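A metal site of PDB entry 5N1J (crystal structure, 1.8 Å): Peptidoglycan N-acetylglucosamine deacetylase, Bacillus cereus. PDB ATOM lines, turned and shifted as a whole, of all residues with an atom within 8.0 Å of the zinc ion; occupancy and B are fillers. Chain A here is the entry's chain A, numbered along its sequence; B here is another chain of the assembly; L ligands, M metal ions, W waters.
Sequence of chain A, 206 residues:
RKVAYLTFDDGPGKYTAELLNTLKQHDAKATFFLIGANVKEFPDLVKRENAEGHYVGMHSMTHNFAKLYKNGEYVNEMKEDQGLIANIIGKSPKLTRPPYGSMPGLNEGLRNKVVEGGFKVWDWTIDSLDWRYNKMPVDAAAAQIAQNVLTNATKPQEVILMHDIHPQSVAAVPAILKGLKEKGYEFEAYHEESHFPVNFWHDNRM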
ATOM      1  N   PHE A   8       1.878  22.749  29.552  1.00  0.00           N
ATOM      2  CA  PHE A   8       1.453  23.287  28.269  1.00  0.00           C
ATOM      3  C   PHE A   8       2.554  24.153  27.663  1.00  0.00           C
ATOM      4  O   PHE A   8       3.003  25.135  28.256  1.00  0.00           O
ATOM      5  CB  PHE A   8       0.143  24.086  28.440  1.00  0.00           C
ATOM      6  CG  PHE A   8      -1.016  23.242  28.920  1.00  0.00           C
ATOM      7  CD1 PHE A   8      -1.749  22.472  28.023  1.00  0.00           C
ATOM      8  CD2 PHE A   8      -1.358  23.205  30.275  1.00  0.00           C
ATOM      9  CE1 PHE A   8      -2.810  21.671  28.462  1.00  0.00           C
ATOM     10  CE2 PHE A   8      -2.412  22.418  30.729  1.00  0.00           C
ATOM     11  CZ  PHE A   8      -3.143  21.641  29.826  1.00  0.00           C
ATOM     12  N   ASP A   9       3.025  23.739  26.482  1.00  0.00           N
ATOM     13  CA  ASP A   9       4.146  24.370  25.793  1.00  0.00           C
ATOM     14  C   ASP A   9       3.700  25.266  24.640  1.00  0.00           C
ATOM     15  O   ASP A   9       2.660  25.017  24.022  1.00  0.00           O
ATOM     16  CB  ASP A   9       5.098  23.304  25.226  1.00  0.00           C
ATOM     17  CG  ASP A   9       5.923  22.588  26.293  1.00  0.00           C
ATOM     18  OD1 ASP A   9       5.668  22.801  27.484  1.00  0.00           O
ATOM     19  OD2 ASP A   9       6.846  21.818  25.905  1.00  0.00           O
ATOM     20  N   ASP A  10       4.535  26.267  24.354  1.00  0.00           N
ATOM     21  CA  ASP A  10       4.558  27.031  23.097  1.00  0.00           C
ATOM     22  C   ASP A  10       3.629  28.241  23.082  1.00  0.00           C
ATOM     23  O   ASP A  10       3.528  28.927  22.064  1.00  0.00           O
ATOM     24  CB  ASP A  10       4.223  26.143  21.875  1.00  0.00           C
ATOM     25  CG  ASP A  10       5.302  25.109  21.553  1.00  0.00           C
ATOM     26  OD1 ASP A  10       6.312  24.957  22.271  1.00  0.00           O
ATOM     27  OD2 ASP A  10       5.119  24.393  20.534  1.00  0.00           O
ATOM     28  N   GLY A  11       2.977  28.516  24.212  1.00  0.00           N
ATOM     29  CA  GLY A  11       2.019  29.607  24.259  1.00  0.00           C
ATOM     30  C   GLY A  11       2.584  30.888  24.850  1.00  0.00           C
ATOM     31  O   GLY A  11       3.808  31.058  24.921  1.00  0.00           O
ATOM     32  N   PHE A  33       4.744  26.681  29.877  1.00  0.00           N
ATOM     33  CA  PHE A  33       6.081  27.033  29.431  1.00  0.00           C
ATOM     34  C   PHE A  33       5.976  27.924  28.190  1.00  0.00           C
ATOM     35  O   PHE A  33       5.563  27.472  27.120  1.00  0.00           O
ATOM     36  CB  PHE A  33       6.904  25.770  29.141  1.00  0.00           C
ATOM     37  CG  PHE A  33       7.213  24.959  30.367  1.00  0.00           C
ATOM     38  CD1 PHE A  33       8.138  25.408  31.310  1.00  0.00           C
ATOM     39  CD2 PHE A  33       6.567  23.761  30.593  1.00  0.00           C
ATOM     40  CE1 PHE A  33       8.423  24.651  32.443  1.00  0.00           C
ATOM     41  CE2 PHE A  33       6.843  22.996  31.718  1.00  0.00           C
ATOM     42  CZ  PHE A  33       7.769  23.452  32.654  1.00  0.00           C
ATOM     43  N   ILE A  35       6.833  30.894  25.193  1.00  0.00           N
ATOM     44  CA  ILE A  35       7.813  31.414  24.237  1.00  0.00           C
ATOM     45  C   ILE A  35       7.808  32.931  24.305  1.00  0.00           C
ATOM     46  O   ILE A  35       6.747  33.551  24.304  1.00  0.00           O
ATOM     47  CB  ILE A  35       7.488  30.930  22.803  1.00  0.00           C
ATOM     48  CG1 ILE A  35       7.747  29.430  22.681  1.00  0.00           C
ATOM     49  CG2 ILE A  35       8.312  31.715  21.780  1.00  0.00           C
ATOM     50  CD1 ILE A  35       7.124  28.811  21.390  1.00  0.00           C
ATOM     51  N   HIS A  59      10.223  28.676  27.798  1.00  0.00           N
ATOM     52  CA  HIS A  59      10.337  27.714  26.690  1.00  0.00           C
ATOM     53  C   HIS A  59      11.168  28.318  25.538  1.00  0.00           C
ATOM     54  O   HIS A  59      11.071  27.869  24.411  1.00  0.00           O
ATOM     55  CB  HIS A  59       8.949  27.295  26.215  1.00  0.00           C
ATOM     56  CG  HIS A  59       8.942  26.056  25.352  1.00  0.00           C
ATOM     57  ND1 HIS A  59       9.671  24.931  25.666  1.00  0.00           N
ATOM     58  CD2 HIS A  59       8.286  25.781  24.202  1.00  0.00           C
ATOM     59  CE1 HIS A  59       9.476  24.006  24.737  1.00  0.00           C
ATOM     60  NE2 HIS A  59       8.624  24.501  23.844  1.00  0.00           N
ATOM     61  N   SER A  60      11.957  29.346  25.883  1.00  0.00           N
ATOM     62  CA  SER A  60      12.954  30.020  25.033  1.00  0.00           C
ATOM     63  C   SER A  60      12.354  31.187  24.238  1.00  0.00           C
ATOM     64  O   SER A  60      11.157  31.484  24.352  1.00  0.00           O
ATOM     65  CB  SER A  60      13.653  29.029  24.064  1.00  0.00           C
ATOM     66  OG  SER A  60      12.893  28.863  22.863  1.00  0.00           O
ATOM     67  N   HIS A  63      12.874  29.125  19.908  1.00  0.00           N
ATOM     68  CA  HIS A  63      12.470  27.733  19.725  1.00  0.00           C
ATOM     69  C   HIS A  63      13.249  27.133  18.557  1.00  0.00           C
ATOM     70  O   HIS A  63      12.737  26.273  17.848  1.00  0.00           O
ATOM     71  CB  HIS A  63      10.952  27.631  19.475  1.00  0.00           C
ATOM     72  CG  HIS A  63      10.359  26.319  19.865  1.00  0.00           C
ATOM     73  ND1 HIS A  63      10.474  25.177  19.101  1.00  0.00           N
ATOM     74  CD2 HIS A  63       9.599  25.968  20.936  1.00  0.00           C
ATOM     75  CE1 HIS A  63       9.827  24.182  19.688  1.00  0.00           C
ATOM     76  NE2 HIS A  63       9.268  24.642  20.786  1.00  0.00           N
ATOM     77  N   ARG A  97      11.771  24.491  30.142  1.00  0.00           N
ATOM     78  CA  ARG A  97      11.363  23.312  29.354  1.00  0.00           C
ATOM     79  C   ARG A  97      12.058  23.426  28.004  1.00  0.00           C
ATOM     80  O   ARG A  97      11.820  24.374  27.255  1.00  0.00           O
ATOM     81  CB  ARG A  97       9.829  23.291  29.235  1.00  0.00           C
ATOM     82  CG  ARG A  97       9.167  22.438  28.131  1.00  0.00           C
ATOM     83  CD  ARG A  97       9.372  20.939  28.294  1.00  0.00           C
ATOM     84  NE  ARG A  97       8.769  20.319  29.482  1.00  0.00           N
ATOM     85  CZ  ARG A  97       7.470  20.122  29.707  1.00  0.00           C
ATOM     86  NH1 ARG A  97       6.550  20.568  28.853  1.00  0.00           N
ATOM     87  NH2 ARG A  97       7.078  19.481  30.798  1.00  0.00           N
ATOM     88  N   PRO A  98      12.960  22.474  27.690  1.00  0.00           N
ATOM     89  CA  PRO A  98      13.755  22.593  26.460  1.00  0.00           C
ATOM     90  C   PRO A  98      12.868  22.418  25.228  1.00  0.00           C
ATOM     91  O   PRO A  98      12.124  21.464  25.184  1.00  0.00           O
ATOM     92  CB  PRO A  98      14.761  21.430  26.546  1.00  0.00           C
ATOM     93  CG  PRO A  98      14.690  20.902  27.923  1.00  0.00           C
ATOM     94  CD  PRO A  98      13.359  21.326  28.526  1.00  0.00           C
ATOM     95  N   PRO A  99      12.956  23.328  24.260  1.00  0.00           N
ATOM     96  CA  PRO A  99      12.324  23.007  22.987  1.00  0.00           C
ATOM     97  C   PRO A  99      12.879  21.682  22.454  1.00  0.00           C
ATOM     98  O   PRO A  99      14.096  21.482  22.492  1.00  0.00           O
ATOM     99  CB  PRO A  99      12.700  24.200  22.085  1.00  0.00           C
ATOM    100  CG  PRO A  99      12.814  25.367  23.092  1.00  0.00           C
ATOM    101  CD  PRO A  99      13.444  24.725  24.322  1.00  0.00           C
ATOM    102  N   TYR A 100      11.980  20.790  22.027  1.00  0.00           N
ATOM    103  CA  TYR A 100      12.330  19.462  21.499  1.00  0.00           C
ATOM    104  C   TYR A 100      12.909  18.508  22.550  1.00  0.00           C
ATOM    105  O   TYR A 100      13.404  17.429  22.200  1.00  0.00           O
ATOM    106  CB  TYR A 100      13.327  19.580  20.328  1.00  0.00           C
ATOM    107  CG  TYR A 100      12.910  20.644  19.326  1.00  0.00           C
ATOM    108  CD1 TYR A 100      11.896  20.392  18.404  1.00  0.00           C
ATOM    109  CD2 TYR A 100      13.526  21.884  19.316  1.00  0.00           C
ATOM    110  CE1 TYR A 100      11.506  21.367  17.488  1.00  0.00           C
ATOM    111  CE2 TYR A 100      13.143  22.860  18.416  1.00  0.00           C
ATOM    112  CZ  TYR A 100      12.138  22.601  17.503  1.00  0.00           C
ATOM    113  OH  TYR A 100      11.753  23.585  16.610  1.00  0.00           O
ATOM    114  N   GLY A 101      12.839  18.875  23.820  1.00  0.00           N
ATOM    115  CA  GLY A 101      13.383  18.034  24.876  1.00  0.00           C
ATOM    116  C   GLY A 101      14.900  18.197  25.016  1.00  0.00           C
ATOM    117  O   GLY A 101      15.566  18.693  24.110  1.00  0.00           O
ATOM    118  N   TRP A 124       9.537  15.553  30.281  1.00  0.00           N
ATOM    119  CA  TRP A 124       8.209  14.991  30.598  1.00  0.00           C
ATOM    120  C   TRP A 124       8.252  13.476  30.761  1.00  0.00           C
ATOM    121  O   TRP A 124       9.228  12.826  30.343  1.00  0.00           O
ATOM    122  CB  TRP A 124       7.182  15.342  29.512  1.00  0.00           C
ATOM    123  CG  TRP A 124       7.680  14.957  28.127  1.00  0.00           C
ATOM    124  CD1 TRP A 124       7.490  13.772  27.480  1.00  0.00           C
ATOM    125  CD2 TRP A 124       8.464  15.768  27.262  1.00  0.00           C
ATOM    126  NE1 TRP A 124       8.103  13.797  26.255  1.00  0.00           N
ATOM    127  CE2 TRP A 124       8.717  15.011  26.094  1.00  0.00           C
ATOM    128  CE3 TRP A 124       8.988  17.074  27.355  1.00  0.00           C
ATOM    129  CZ2 TRP A 124       9.473  15.524  25.025  1.00  0.00           C
ATOM    130  CZ3 TRP A 124       9.744  17.566  26.293  1.00  0.00           C
ATOM    131  CH2 TRP A 124       9.962  16.795  25.149  1.00  0.00           C
ATOM    132  N   LEU A 161       3.125  16.236  28.681  1.00  0.00           N
ATOM    133  CA  LEU A 161       3.436  17.225  27.657  1.00  0.00           C
ATOM    134  C   LEU A 161       2.244  17.453  26.760  1.00  0.00           C
ATOM    135  O   LEU A 161       1.811  16.518  26.075  1.00  0.00           O
ATOM    136  CB  LEU A 161       4.623  16.769  26.791  1.00  0.00           C
ATOM    137  CG  LEU A 161       4.921  17.608  25.526  1.00  0.00           C
ATOM    138  CD1 LEU A 161       5.306  19.036  25.920  1.00  0.00           C
ATOM    139  CD2 LEU A 161       6.003  16.980  24.645  1.00  0.00           C
ATOM    140  N   MET A 162       1.729  18.684  26.763  1.00  0.00           N
ATOM    141  CA  MET A 162       0.753  19.131  25.777  1.00  0.00           C
ATOM    142  C   MET A 162       1.121  20.512  25.220  1.00  0.00           C
ATOM    143  O   MET A 162       2.030  21.165  25.729  1.00  0.00           O
ATOM    144  CB  MET A 162      -0.653  19.165  26.385  1.00  0.00           C
ATOM    145  CG  MET A 162      -1.060  17.820  26.984  1.00  0.00           C
ATOM    146  SD  MET A 162      -2.745  17.830  27.620  1.00  0.00           S
ATOM    147  CE  MET A 162      -3.691  17.736  26.095  1.00  0.00           C
ATOM    148  N   HIS A 163       0.420  20.940  24.177  1.00  0.00           N
ATOM    149  CA  HIS A 163       0.640  22.269  23.602  1.00  0.00           C
ATOM    150  C   HIS A 163      -0.675  23.034  23.586  1.00  0.00           C
ATOM    151  O   HIS A 163      -1.610  22.608  22.914  1.00  0.00           O
ATOM    152  CB  HIS A 163       1.229  22.139  22.197  1.00  0.00           C
ATOM    153  CG  HIS A 163       2.489  21.342  22.132  1.00  0.00           C
ATOM    154  ND1 HIS A 163       2.497  19.961  22.082  1.00  0.00           N
ATOM    155  CD2 HIS A 163       3.792  21.730  22.132  1.00  0.00           C
ATOM    156  CE1 HIS A 163       3.752  19.526  22.055  1.00  0.00           C
ATOM    157  NE2 HIS A 163       4.549  20.579  22.077  1.00  0.00           N
ATOM    158  N   ILE A 165      -1.431  25.650  22.200  1.00  0.00           N
ATOM    159  CA  ILE A 165      -1.626  26.326  20.920  1.00  0.00           C
ATOM    160  C   ILE A 165      -2.363  25.439  19.896  1.00  0.00           C
ATOM    161  O   ILE A 165      -2.734  25.921  18.819  1.00  0.00           O
ATOM    162  CB  ILE A 165      -0.296  26.780  20.332  1.00  0.00           C
ATOM    163  CG1 ILE A 165       0.628  25.571  20.153  1.00  0.00           C
ATOM    164  CG2 ILE A 165       0.345  27.825  21.254  1.00  0.00           C
ATOM    165  CD1 ILE A 165       1.801  25.813  19.226  1.00  0.00           C
ATOM    166  N   HIS B 202       7.542  17.736  14.597  1.00  0.00           N
ATOM    167  CA  HIS B 202       6.110  17.626  14.924  1.00  0.00           C
ATOM    168  C   HIS B 202       5.254  18.068  13.730  1.00  0.00           C
ATOM    169  O   HIS B 202       4.252  18.751  13.897  1.00  0.00           O
ATOM    170  CB  HIS B 202       5.769  18.455  16.174  1.00  0.00           C
ATOM    171  CG  HIS B 202       6.197  17.811  17.453  1.00  0.00           C
ATOM    172  ND1 HIS B 202       5.846  18.321  18.689  1.00  0.00           N
ATOM    173  CD2 HIS B 202       6.949  16.712  17.698  1.00  0.00           C
ATOM    174  CE1 HIS B 202       6.359  17.546  19.635  1.00  0.00           C
ATOM    175  NE2 HIS B 202       7.036  16.575  19.057  1.00  0.00           N
HETATM  176  C1  LIG L   1       8.379  21.211  23.129  1.00  0.00           C
HETATM  177  O1  LIG L   1       7.318  21.872  23.293  1.00  0.00           O
HETATM  178  O2  LIG L   1       9.174  21.625  22.250  1.00  0.00           O
HETATM  179  C2  LIG L   1       8.687  19.976  23.922  1.00  0.00           C
HETATM  180 ZN    ZN M   1       7.943  23.596  22.076  1.00  0.00          ZN
HETATM  181  O   HOH W   1       6.944  22.522  20.455  1.00  0.00           O
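O of Arg 97 sits at hydrogen-bond distance from ND1 of His 59. The backbone carbonyl oxygen of His 63 sits at hydrogen-bond distance from the side-chain hydroxyl of Tyr 100 (3.1 Å). The backbone NH (N) of His 63 is in hydrogen-bond range of the side-chain hydroxyl (OG) of Ser 60, 3.0 Å away. The backbone carbonyl oxygen of Phe 33 is in hydrogen-bond range of the backbone NH of Asp 10.
NE2 of His 59 is bound to the zinc ion (2.1 Å). The zinc ion is bound by NE2 of His 63 (2.1 Å). The side-chain carboxylate (OD1) of Asp 10 binds the zinc ion. Water W1 binds the zinc ion, 2.2 Å away. O1 of the ligand binds the zinc ion (2.2 Å). O2 of the ligand is bound to the zinc ion (2.3 Å). The zinc ion has six donor atoms within binding distance.
Water W1 lies within hydrogen-bond range of the side-chain carboxylate of Asp 10 (2.6 Å) and a ring nitrogen (NE2) of His 163 (3.5 Å).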
